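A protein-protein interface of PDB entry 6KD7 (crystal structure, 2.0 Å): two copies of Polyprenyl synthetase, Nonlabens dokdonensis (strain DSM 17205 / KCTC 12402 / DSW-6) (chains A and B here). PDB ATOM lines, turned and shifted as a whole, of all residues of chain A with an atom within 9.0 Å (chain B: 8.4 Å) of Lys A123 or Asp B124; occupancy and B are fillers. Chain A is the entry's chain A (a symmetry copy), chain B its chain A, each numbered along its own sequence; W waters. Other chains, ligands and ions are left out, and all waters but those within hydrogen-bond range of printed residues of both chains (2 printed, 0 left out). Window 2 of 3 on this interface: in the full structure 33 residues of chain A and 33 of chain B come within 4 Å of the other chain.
Water W1 bridges the side-chain carboxylate of Glu A119 and the backbone carbonyl oxygen of Lys B131. Water W2 bridges the side-chain carboxylate of Glu A119 and the backbone carbonyl oxygen of Asn B130.
The backbone NH of Asp B124 is in hydrogen-bond range of the side-chain carboxylate of Asp B122, 3.1 Å away. The side-chain carboxylate of Asp A122 sits at hydrogen-bond distance from the backbone NH of Asp A124, at 3.1 Å. The side-chain carboxylate of Asp B124 sits close to the side-chain amide oxygen of Gln B128 (3.4 Å). O of Phe A126 lies close to OD1 of Asn A130, at 3.0 Å. The backbone carbonyl oxygen (O) of Phe B126 sits close to the side-chain amide oxygen (OD1) of Asn B130. OE1 of Gln A128 lies close to OD2 of Asp A124 (3.4 Å).
Hydrophobic or aromatic side chains of chain A that line the printed part of chain B: Phe A126 and Tyr A127. Hydrophobic or aromatic side chains of chain B that line the printed part of chain A: Phe B126 and Tyr B127. Along chain B the printed residues that touch a printed residue of chain A span positions 123 to 131.
Of the printed residues of chain B, Lys A123 touches Asp B124 and Tyr B127. Asp B124 touches just one residue of chain A: Lys A123 (3.0 Å). Printed residues of chain A within 4 Å of Lys B123: Asp A124 (3.0 Å) and Tyr A127 (3.99 Å). Printed residues of chain A within 4 Å of Asn B130: Phe A126 and Asn A130. Of the printed residues of chain B, Asn A130 touches Phe B126 (3.6 Å) and Asn B130 (3.5 Å). Of the printed residues of chain A, Lys B131 touches Glu A119 (3.8 Å). Of the printed residues of chain B, Phe A126 touches Phe B126 (3.4 Å), Tyr B127 (3.6 Å) and Asn B130 (3.6 Å).
Among the printed residues, merely in contact across the chains: Glu A119 with Lys B131, Lys A123 with Asp B124, Lys A123 with Tyr B127, Asp A124 with Lys B123, Phe A126 with Phe B126, Phe A126 with Tyr B127, Phe A126 with Asn B130, Tyr A127 with Lys B123, Tyr A127 with Phe B126, Asn A130 with Phe B126 and Asn A130 with Asn B130.
OH of Tyr B127 is in hydrogen-bond range of O of Glu A119, at 2.7 Å.
Lys A123 touches Asp B124, and with the chains exchanged Asp A124 touches Lys B123. Lys A123 touches Tyr B127, and with the chains exchanged Tyr A127 touches Lys B123. Phe B126 touches its own counterpart, Phe A126. Asn B130 touches its own counterpart, Asn A130. Of the 12 pairs that touch across the chains among the printed residues, 10 have their exchanged pair printed and touching as well.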
ATOM      1  N   PHE A 118     -16.107  -0.201  26.371  1.00  0.00           N
ATOM      2  CA  PHE A 118     -16.516  -0.142  24.955  1.00  0.00           C
ATOM      3  C   PHE A 118     -18.013  -0.495  24.807  1.00  0.00           C
ATOM      4  O   PHE A 118     -18.548  -0.259  23.749  1.00  0.00           O
ATOM      5  CB  PHE A 118     -15.653  -1.051  24.094  1.00  0.00           C
ATOM      6  CG  PHE A 118     -14.214  -0.670  24.089  1.00  0.00           C
ATOM      7  CD1 PHE A 118     -13.832   0.651  24.045  1.00  0.00           C
ATOM      8  CD2 PHE A 118     -13.219  -1.625  24.107  1.00  0.00           C
ATOM      9  CE1 PHE A 118     -12.496   1.016  24.041  1.00  0.00           C
ATOM     10  CE2 PHE A 118     -11.882  -1.254  24.139  1.00  0.00           C
ATOM     11  CZ  PHE A 118     -11.519   0.068  24.104  1.00  0.00           C
ATOM     12  N   GLU A 119     -18.673  -1.046  25.811  1.00  0.00           N
ATOM     13  CA  GLU A 119     -19.972  -1.756  25.608  1.00  0.00           C
ATOM     14  C   GLU A 119     -21.113  -0.811  25.203  1.00  0.00           C
ATOM     15  O   GLU A 119     -22.031  -1.340  24.571  1.00  0.00           O
ATOM     16  CB  GLU A 119     -20.384  -2.578  26.833  1.00  0.00           C
ATOM     17  CG  GLU A 119     -19.541  -3.834  26.936  1.00  0.00           C
ATOM     18  CD  GLU A 119     -19.600  -4.626  28.225  1.00  0.00           C
ATOM     19  OE1 GLU A 119     -20.509  -4.367  29.007  1.00  0.00           O
ATOM     20  OE2 GLU A 119     -18.825  -5.619  28.341  1.00  0.00           O
ATOM     21  N   ASP A 120     -21.083   0.487  25.541  1.00  0.00           N
ATOM     22  CA  ASP A 120     -22.145   1.446  25.117  1.00  0.00           C
ATOM     23  C   ASP A 120     -22.017   1.819  23.637  1.00  0.00           C
ATOM     24  O   ASP A 120     -22.953   2.378  23.157  1.00  0.00           O
ATOM     25  CB  ASP A 120     -22.183   2.735  25.927  1.00  0.00           C
ATOM     26  CG  ASP A 120     -22.640   2.474  27.331  1.00  0.00           C
ATOM     27  OD1 ASP A 120     -23.148   1.369  27.573  1.00  0.00           O
ATOM     28  OD2 ASP A 120     -22.456   3.348  28.160  1.00  0.00           O
ATOM     29  N   TYR A 121     -20.927   1.482  22.959  1.00  0.00           N
ATOM     30  CA  TYR A 121     -20.814   1.830  21.522  1.00  0.00           C
ATOM     31  C   TYR A 121     -21.694   0.919  20.657  1.00  0.00           C
ATOM     32  O   TYR A 121     -22.051  -0.176  21.091  1.00  0.00           O
ATOM     33  CB  TYR A 121     -19.351   1.931  21.089  1.00  0.00           C
ATOM     34  CG  TYR A 121     -18.648   3.077  21.762  1.00  0.00           C
ATOM     35  CD1 TYR A 121     -18.860   4.378  21.353  1.00  0.00           C
ATOM     36  CD2 TYR A 121     -17.835   2.872  22.860  1.00  0.00           C
ATOM     37  CE1 TYR A 121     -18.247   5.442  21.987  1.00  0.00           C
ATOM     38  CE2 TYR A 121     -17.223   3.926  23.510  1.00  0.00           C
ATOM     39  CZ  TYR A 121     -17.428   5.218  23.073  1.00  0.00           C
ATOM     40  OH  TYR A 121     -16.828   6.257  23.704  1.00  0.00           O
ATOM     41  N   ASP A 122     -22.086   1.417  19.487  1.00  0.00           N
ATOM     42  CA  ASP A 122     -22.880   0.619  18.518  1.00  0.00           C
ATOM     43  C   ASP A 122     -21.986  -0.548  18.079  1.00  0.00           C
ATOM     44  O   ASP A 122     -20.755  -0.437  18.240  1.00  0.00           O
ATOM     45  CB  ASP A 122     -23.435   1.485  17.371  1.00  0.00           C
ATOM     46  CG  ASP A 122     -22.423   2.008  16.371  1.00  0.00           C
ATOM     47  OD1 ASP A 122     -21.525   1.258  15.924  1.00  0.00           O
ATOM     48  OD2 ASP A 122     -22.550   3.176  16.005  1.00  0.00           O
ATOM     49  N   LYS A 123     -22.590  -1.597  17.519  1.00  0.00           N
ATOM     50  CA  LYS A 123     -21.960  -2.906  17.246  1.00  0.00           C
ATOM     51  C   LYS A 123     -20.827  -2.689  16.271  1.00  0.00           C
ATOM     52  O   LYS A 123     -19.832  -3.421  16.307  1.00  0.00           O
ATOM     53  CB  LYS A 123     -23.011  -3.906  16.749  1.00  0.00           C
ATOM     54  CG  LYS A 123     -23.850  -4.502  17.880  1.00  0.00           C
ATOM     55  CD  LYS A 123     -25.155  -5.202  17.468  1.00  0.00           C
ATOM     56  CE  LYS A 123     -26.012  -5.642  18.651  1.00  0.00           C
ATOM     57  NZ  LYS A 123     -25.884  -4.760  19.847  1.00  0.00           N
ATOM     58  N   ASP A 124     -20.966  -1.732  15.381  1.00  0.00           N
ATOM     59  CA  ASP A 124     -19.921  -1.528  14.354  1.00  0.00           C
ATOM     60  C   ASP A 124     -18.673  -0.882  15.020  1.00  0.00           C
ATOM     61  O   ASP A 124     -17.536  -1.235  14.711  1.00  0.00           O
ATOM     62  CB  ASP A 124     -20.473  -0.717  13.185  1.00  0.00           C
ATOM     63  CG  ASP A 124     -19.545  -0.897  11.999  1.00  0.00           C
ATOM     64  OD1 ASP A 124     -19.596  -1.994  11.350  1.00  0.00           O
ATOM     65  OD2 ASP A 124     -18.726   0.011  11.773  1.00  0.00           O
ATOM     66  N   LYS A 125     -18.870   0.110  15.870  1.00  0.00           N
ATOM     67  CA  LYS A 125     -17.727   0.814  16.478  1.00  0.00           C
ATOM     68  C   LYS A 125     -17.117  -0.096  17.563  1.00  0.00           C
ATOM     69  O   LYS A 125     -15.894  -0.184  17.642  1.00  0.00           O
ATOM     70  CB  LYS A 125     -18.252   2.140  17.002  1.00  0.00           C
ATOM     71  CG  LYS A 125     -18.452   3.171  15.912  1.00  0.00           C
ATOM     72  CD  LYS A 125     -19.229   4.328  16.451  1.00  0.00           C
ATOM     73  CE  LYS A 125     -19.573   5.289  15.325  1.00  0.00           C
ATOM     74  NZ  LYS A 125     -20.219   6.448  15.947  1.00  0.00           N
ATOM     75  N   PHE A 126     -17.974  -0.715  18.363  1.00  0.00           N
ATOM     76  CA  PHE A 126     -17.595  -1.755  19.343  1.00  0.00           C
ATOM     77  C   PHE A 126     -16.609  -2.724  18.714  1.00  0.00           C
ATOM     78  O   PHE A 126     -15.514  -2.890  19.253  1.00  0.00           O
ATOM     79  CB  PHE A 126     -18.793  -2.533  19.841  1.00  0.00           C
ATOM     80  CG  PHE A 126     -18.425  -3.514  20.916  1.00  0.00           C
ATOM     81  CD1 PHE A 126     -18.390  -3.119  22.252  1.00  0.00           C
ATOM     82  CD2 PHE A 126     -18.095  -4.817  20.571  1.00  0.00           C
ATOM     83  CE1 PHE A 126     -18.086  -4.042  23.240  1.00  0.00           C
ATOM     84  CE2 PHE A 126     -17.794  -5.736  21.568  1.00  0.00           C
ATOM     85  CZ  PHE A 126     -17.790  -5.354  22.895  1.00  0.00           C
ATOM     86  N   TYR A 127     -16.934  -3.248  17.544  1.00  0.00           N
ATOM     87  CA  TYR A 127     -16.059  -4.204  16.850  1.00  0.00           C
ATOM     88  C   TYR A 127     -14.733  -3.526  16.522  1.00  0.00           C
ATOM     89  O   TYR A 127     -13.652  -4.132  16.597  1.00  0.00           O
ATOM     90  CB  TYR A 127     -16.731  -4.843  15.624  1.00  0.00           C
ATOM     91  CG  TYR A 127     -15.868  -5.864  14.940  1.00  0.00           C
ATOM     92  CD1 TYR A 127     -15.898  -7.188  15.335  1.00  0.00           C
ATOM     93  CD2 TYR A 127     -14.979  -5.503  13.958  1.00  0.00           C
ATOM     94  CE1 TYR A 127     -15.096  -8.140  14.737  1.00  0.00           C
ATOM     95  CE2 TYR A 127     -14.157  -6.436  13.359  1.00  0.00           C
ATOM     96  CZ  TYR A 127     -14.224  -7.757  13.758  1.00  0.00           C
ATOM     97  OH  TYR A 127     -13.393  -8.663  13.188  1.00  0.00           O
ATOM     98  N   GLN A 128     -14.774  -2.315  16.030  1.00  0.00           N
ATOM     99  CA  GLN A 128     -13.541  -1.700  15.482  1.00  0.00           C
ATOM    100  C   GLN A 128     -12.613  -1.326  16.662  1.00  0.00           C
ATOM    101  O   GLN A 128     -11.385  -1.408  16.507  1.00  0.00           O
ATOM    102  CB  GLN A 128     -13.955  -0.490  14.632  1.00  0.00           C
ATOM    103  CG  GLN A 128     -14.408  -0.831  13.213  1.00  0.00           C
ATOM    104  CD  GLN A 128     -14.661   0.471  12.484  1.00  0.00           C
ATOM    105  OE1 GLN A 128     -15.679   1.125  12.686  1.00  0.00           O
ATOM    106  NE2 GLN A 128     -13.651   0.943  11.781  1.00  0.00           N
ATOM    107  N   LEU A 129     -13.213  -0.809  17.729  1.00  0.00           N
ATOM    108  CA  LEU A 129     -12.543  -0.357  18.972  1.00  0.00           C
ATOM    109  C   LEU A 129     -11.826  -1.584  19.567  1.00  0.00           C
ATOM    110  O   LEU A 129     -10.592  -1.498  19.754  1.00  0.00           O
ATOM    111  CB  LEU A 129     -13.582   0.237  19.924  1.00  0.00           C
ATOM    112  CG  LEU A 129     -14.111   1.627  19.544  1.00  0.00           C
ATOM    113  CD1 LEU A 129     -15.164   2.081  20.530  1.00  0.00           C
ATOM    114  CD2 LEU A 129     -12.985   2.675  19.421  1.00  0.00           C
ATOM    115  N   ASN A 130     -12.559  -2.691  19.761  1.00  0.00           N
ATOM    116  CA  ASN A 130     -12.012  -3.923  20.390  1.00  0.00           C
ATOM    117  C   ASN A 130     -10.840  -4.389  19.560  1.00  0.00           C
ATOM    118  O   ASN A 130      -9.773  -4.695  20.100  1.00  0.00           O
ATOM    119  CB  ASN A 130     -13.014  -5.054  20.548  1.00  0.00           C
ATOM    120  CG  ASN A 130     -13.778  -4.883  21.816  1.00  0.00           C
ATOM    121  OD1 ASN A 130     -14.804  -4.188  21.830  1.00  0.00           O
ATOM    122  ND2 ASN A 130     -13.313  -5.528  22.877  1.00  0.00           N
ATOM    123  N   ILE A 182     -12.477   6.393  15.013  1.00  0.00           N
ATOM    124  CA  ILE A 182     -13.501   5.330  14.868  1.00  0.00           C
ATOM    125  C   ILE A 182     -14.812   5.876  15.415  1.00  0.00           C
ATOM    126  O   ILE A 182     -15.846   5.630  14.832  1.00  0.00           O
ATOM    127  CB  ILE A 182     -13.105   4.045  15.621  1.00  0.00           C
ATOM    128  CG1 ILE A 182     -11.975   3.311  14.904  1.00  0.00           C
ATOM    129  CG2 ILE A 182     -14.312   3.148  15.869  1.00  0.00           C
ATOM    130  CD1 ILE A 182     -11.327   2.280  15.798  1.00  0.00           C
ATOM    131  N   TYR B 121     -16.174 -13.723  14.531  1.00  0.00           N
ATOM    132  CA  TYR B 121     -17.652 -13.767  14.651  1.00  0.00           C
ATOM    133  C   TYR B 121     -18.297 -12.516  14.042  1.00  0.00           C
ATOM    134  O   TYR B 121     -17.632 -11.490  13.906  1.00  0.00           O
ATOM    135  CB  TYR B 121     -18.082 -14.097  16.079  1.00  0.00           C
ATOM    136  CG  TYR B 121     -17.677 -15.490  16.476  1.00  0.00           C
ATOM    137  CD1 TYR B 121     -18.371 -16.589  16.012  1.00  0.00           C
ATOM    138  CD2 TYR B 121     -16.555 -15.716  17.248  1.00  0.00           C
ATOM    139  CE1 TYR B 121     -17.986 -17.876  16.341  1.00  0.00           C
ATOM    140  CE2 TYR B 121     -16.151 -16.995  17.577  1.00  0.00           C
ATOM    141  CZ  TYR B 121     -16.869 -18.082  17.123  1.00  0.00           C
ATOM    142  OH  TYR B 121     -16.483 -19.341  17.445  1.00  0.00           O
ATOM    143  N   ASP B 122     -19.553 -12.647  13.621  1.00  0.00           N
ATOM    144  CA  ASP B 122     -20.326 -11.500  13.078  1.00  0.00           C
ATOM    145  C   ASP B 122     -20.484 -10.498  14.228  1.00  0.00           C
ATOM    146  O   ASP B 122     -20.340 -10.914  15.394  1.00  0.00           O
ATOM    147  CB  ASP B 122     -21.643 -11.950  12.418  1.00  0.00           C
ATOM    148  CG  ASP B 122     -22.726 -12.457  13.350  1.00  0.00           C
ATOM    149  OD1 ASP B 122     -22.984 -11.849  14.413  1.00  0.00           O
ATOM    150  OD2 ASP B 122     -23.346 -13.458  12.994  1.00  0.00           O
ATOM    151  N   LYS B 123     -20.799  -9.244  13.900  1.00  0.00           N
ATOM    152  CA  LYS B 123     -20.765  -8.083  14.814  1.00  0.00           C
ATOM    153  C   LYS B 123     -21.753  -8.332  15.930  1.00  0.00           C
ATOM    154  O   LYS B 123     -21.544  -7.868  17.055  1.00  0.00           O
ATOM    155  CB  LYS B 123     -21.034  -6.788  14.037  1.00  0.00           C
ATOM    156  CG  LYS B 123     -19.806  -6.279  13.282  1.00  0.00           C
ATOM    157  CD  LYS B 123     -20.063  -5.232  12.186  1.00  0.00           C
ATOM    158  CE  LYS B 123     -18.819  -4.878  11.377  1.00  0.00           C
ATOM    159  NZ  LYS B 123     -17.850  -6.004  11.239  1.00  0.00           N
ATOM    160  N   ASP B 124     -22.836  -9.017  15.640  1.00  0.00           N
ATOM    161  CA  ASP B 124     -23.873  -9.222  16.675  1.00  0.00           C
ATOM    162  C   ASP B 124     -23.358 -10.261  17.710  1.00  0.00           C
ATOM    163  O   ASP B 124     -23.569 -10.114  18.914  1.00  0.00           O
ATOM    164  CB  ASP B 124     -25.200  -9.615  16.031  1.00  0.00           C
ATOM    165  CG  ASP B 124     -26.306  -9.396  17.043  1.00  0.00           C
ATOM    166  OD1 ASP B 124     -26.693  -8.201  17.270  1.00  0.00           O
ATOM    167  OD2 ASP B 124     -26.722 -10.394  17.658  1.00  0.00           O
ATOM    168  N   LYS B 125     -22.754 -11.343  17.253  1.00  0.00           N
ATOM    169  CA  LYS B 125     -22.309 -12.401  18.179  1.00  0.00           C
ATOM    170  C   LYS B 125     -21.042 -11.909  18.905  1.00  0.00           C
ATOM    171  O   LYS B 125     -20.934 -12.117  20.111  1.00  0.00           O
ATOM    172  CB  LYS B 125     -22.101 -13.657  17.349  1.00  0.00           C
ATOM    173  CG  LYS B 125     -23.398 -14.354  16.994  1.00  0.00           C
ATOM    174  CD  LYS B 125     -23.139 -15.396  15.954  1.00  0.00           C
ATOM    175  CE  LYS B 125     -24.455 -15.988  15.478  1.00  0.00           C
ATOM    176  NZ  LYS B 125     -24.115 -17.078  14.560  1.00  0.00           N
ATOM    177  N   PHE B 126     -20.131 -11.301  18.158  1.00  0.00           N
ATOM    178  CA  PHE B 126     -18.939 -10.612  18.693  1.00  0.00           C
ATOM    179  C   PHE B 126     -19.325  -9.776  19.902  1.00  0.00           C
ATOM    180  O   PHE B 126     -18.753  -9.981  20.972  1.00  0.00           O
ATOM    181  CB  PHE B 126     -18.290  -9.711  17.665  1.00  0.00           C
ATOM    182  CG  PHE B 126     -17.020  -9.095  18.173  1.00  0.00           C
ATOM    183  CD1 PHE B 126     -15.805  -9.768  18.043  1.00  0.00           C
ATOM    184  CD2 PHE B 126     -17.060  -7.856  18.798  1.00  0.00           C
ATOM    185  CE1 PHE B 126     -14.633  -9.173  18.480  1.00  0.00           C
ATOM    186  CE2 PHE B 126     -15.879  -7.267  19.231  1.00  0.00           C
ATOM    187  CZ  PHE B 126     -14.672  -7.919  19.073  1.00  0.00           C
ATOM    188  N   TYR B 127     -20.350  -8.951  19.769  1.00  0.00           N
ATOM    189  CA  TYR B 127     -20.804  -8.089  20.869  1.00  0.00           C
ATOM    190  C   TYR B 127     -21.263  -8.960  22.034  1.00  0.00           C
ATOM    191  O   TYR B 127     -21.044  -8.643  23.214  1.00  0.00           O
ATOM    192  CB  TYR B 127     -21.861  -7.065  20.426  1.00  0.00           C
ATOM    193  CG  TYR B 127     -22.290  -6.141  21.528  1.00  0.00           C
ATOM    194  CD1 TYR B 127     -21.608  -4.962  21.763  1.00  0.00           C
ATOM    195  CD2 TYR B 127     -23.320  -6.471  22.375  1.00  0.00           C
ATOM    196  CE1 TYR B 127     -21.970  -4.108  22.787  1.00  0.00           C
ATOM    197  CE2 TYR B 127     -23.687  -5.639  23.414  1.00  0.00           C
ATOM    198  CZ  TYR B 127     -23.002  -4.455  23.611  1.00  0.00           C
ATOM    199  OH  TYR B 127     -23.346  -3.658  24.651  1.00  0.00           O
ATOM    200  N   GLN B 128     -22.015  -9.994  21.761  1.00  0.00           N
ATOM    201  CA  GLN B 128     -22.676 -10.737  22.861  1.00  0.00           C
ATOM    202  C   GLN B 128     -21.602 -11.557  23.615  1.00  0.00           C
ATOM    203  O   GLN B 128     -21.723 -11.721  24.838  1.00  0.00           O
ATOM    204  CB  GLN B 128     -23.780 -11.609  22.246  1.00  0.00           C
ATOM    205  CG  GLN B 128     -25.090 -10.875  21.963  1.00  0.00           C
ATOM    206  CD  GLN B 128     -26.096 -11.898  21.477  1.00  0.00           C
ATOM    207  OE1 GLN B 128     -26.055 -12.334  20.331  1.00  0.00           O
ATOM    208  NE2 GLN B 128     -26.877 -12.420  22.400  1.00  0.00           N
ATOM    209  N   LEU B 129     -20.683 -12.144  22.855  1.00  0.00           N
ATOM    210  CA  LEU B 129     -19.568 -12.994  23.336  1.00  0.00           C
ATOM    211  C   LEU B 129     -18.706 -12.119  24.265  1.00  0.00           C
ATOM    212  O   LEU B 129     -18.531 -12.517  25.437  1.00  0.00           O
ATOM    213  CB  LEU B 129     -18.784 -13.531  22.137  1.00  0.00           C
ATOM    214  CG  LEU B 129     -19.471 -14.651  21.343  1.00  0.00           C
ATOM    215  CD1 LEU B 129     -18.622 -15.059  20.160  1.00  0.00           C
ATOM    216  CD2 LEU B 129     -19.815 -15.872  22.221  1.00  0.00           C
ATOM    217  N   ASN B 130     -18.275 -10.944  23.779  1.00  0.00           N
ATOM    218  CA  ASN B 130     -17.380 -10.033  24.542  1.00  0.00           C
ATOM    219  C   ASN B 130     -18.074  -9.674  25.834  1.00  0.00           C
ATOM    220  O   ASN B 130     -17.469  -9.740  26.908  1.00  0.00           O
ATOM    221  CB  ASN B 130     -16.982  -8.767  23.801  1.00  0.00           C
ATOM    222  CG  ASN B 130     -15.792  -9.033  22.944  1.00  0.00           C
ATOM    223  OD1 ASN B 130     -15.943  -9.467  21.793  1.00  0.00           O
ATOM    224  ND2 ASN B 130     -14.608  -8.756  23.474  1.00  0.00           N
ATOM    225  N   LYS B 131     -19.353  -9.335  25.752  1.00  0.00           N
ATOM    226  CA  LYS B 131     -20.095  -8.883  26.952  1.00  0.00           C
ATOM    227  C   LYS B 131     -20.194  -9.962  28.039  1.00  0.00           C
ATOM    228  O   LYS B 131     -19.863  -9.651  29.162  1.00  0.00           O
ATOM    229  CB  LYS B 131     -21.489  -8.421  26.532  1.00  0.00           C
ATOM    230  CG  LYS B 131     -22.229  -7.596  27.568  1.00  0.00           C
ATOM    231  CD  LYS B 131     -23.207  -6.656  26.937  1.00  0.00           C
ATOM    232  CE  LYS B 131     -23.953  -5.815  27.944  1.00  0.00           C
ATOM    233  NZ  LYS B 131     -24.485  -6.638  29.047  1.00  0.00           N
ATOM    234  N   ILE B 182     -24.940 -18.563  22.170  1.00  0.00           N
ATOM    235  CA  ILE B 182     -24.853 -17.291  21.411  1.00  0.00           C
ATOM    236  C   ILE B 182     -24.454 -17.634  19.984  1.00  0.00           C
ATOM    237  O   ILE B 182     -24.978 -17.041  19.064  1.00  0.00           O
ATOM    238  CB  ILE B 182     -23.827 -16.323  22.032  1.00  0.00           C
ATOM    239  CG1 ILE B 182     -24.351 -15.724  23.335  1.00  0.00           C
ATOM    240  CG2 ILE B 182     -23.395 -15.253  21.036  1.00  0.00           C
ATOM    241  CD1 ILE B 182     -23.241 -15.084  24.137  1.00  0.00           C
ATOM    242  N   GLY B 185     -27.270 -18.742  17.850  1.00  0.00           N
ATOM    243  CA  GLY B 185     -28.246 -17.674  17.576  1.00  0.00           C
ATOM    244  C   GLY B 185     -29.390 -17.731  18.554  1.00  0.00           C
ATOM    245  O   GLY B 185     -30.424 -17.090  18.352  1.00  0.00           O
ATOM    246  N   VAL B 186     -29.250 -18.452  19.639  1.00  0.00           N
ATOM    247  CA  VAL B 186     -30.374 -18.569  20.610  1.00  0.00           C
ATOM    248  C   VAL B 186     -30.622 -17.206  21.260  1.00  0.00           C
ATOM    249  O   VAL B 186     -29.698 -16.408  21.309  1.00  0.00           O
ATOM    250  CB  VAL B 186     -29.973 -19.681  21.593  1.00  0.00           C
ATOM    251  CG1 VAL B 186     -30.581 -19.563  22.963  1.00  0.00           C
ATOM    252  CG2 VAL B 186     -30.264 -21.025  20.974  1.00  0.00           C
ATOM    253  N   GLN B 191     -30.371 -18.410  26.555  1.00  0.00           N
ATOM    254  CA  GLN B 191     -28.943 -18.302  26.925  1.00  0.00           C
ATOM    255  C   GLN B 191     -28.830 -18.340  28.447  1.00  0.00           C
ATOM    256  O   GLN B 191     -28.025 -19.075  28.940  1.00  0.00           O
ATOM    257  CB  GLN B 191     -28.422 -16.948  26.468  1.00  0.00           C
ATOM    258  CG  GLN B 191     -28.058 -16.894  25.004  1.00  0.00           C
ATOM    259  CD  GLN B 191     -27.539 -15.525  24.656  1.00  0.00           C
ATOM    260  OE1 GLN B 191     -26.903 -14.866  25.458  1.00  0.00           O
ATOM    261  NE2 GLN B 191     -27.832 -15.092  23.455  1.00  0.00           N
HETATM  262  O   HOH W   1     -19.578  -7.197  30.312  1.00  0.00           O
HETATM  263  O   HOH W   2     -16.758  -6.529  26.701  1.00  0.00           O
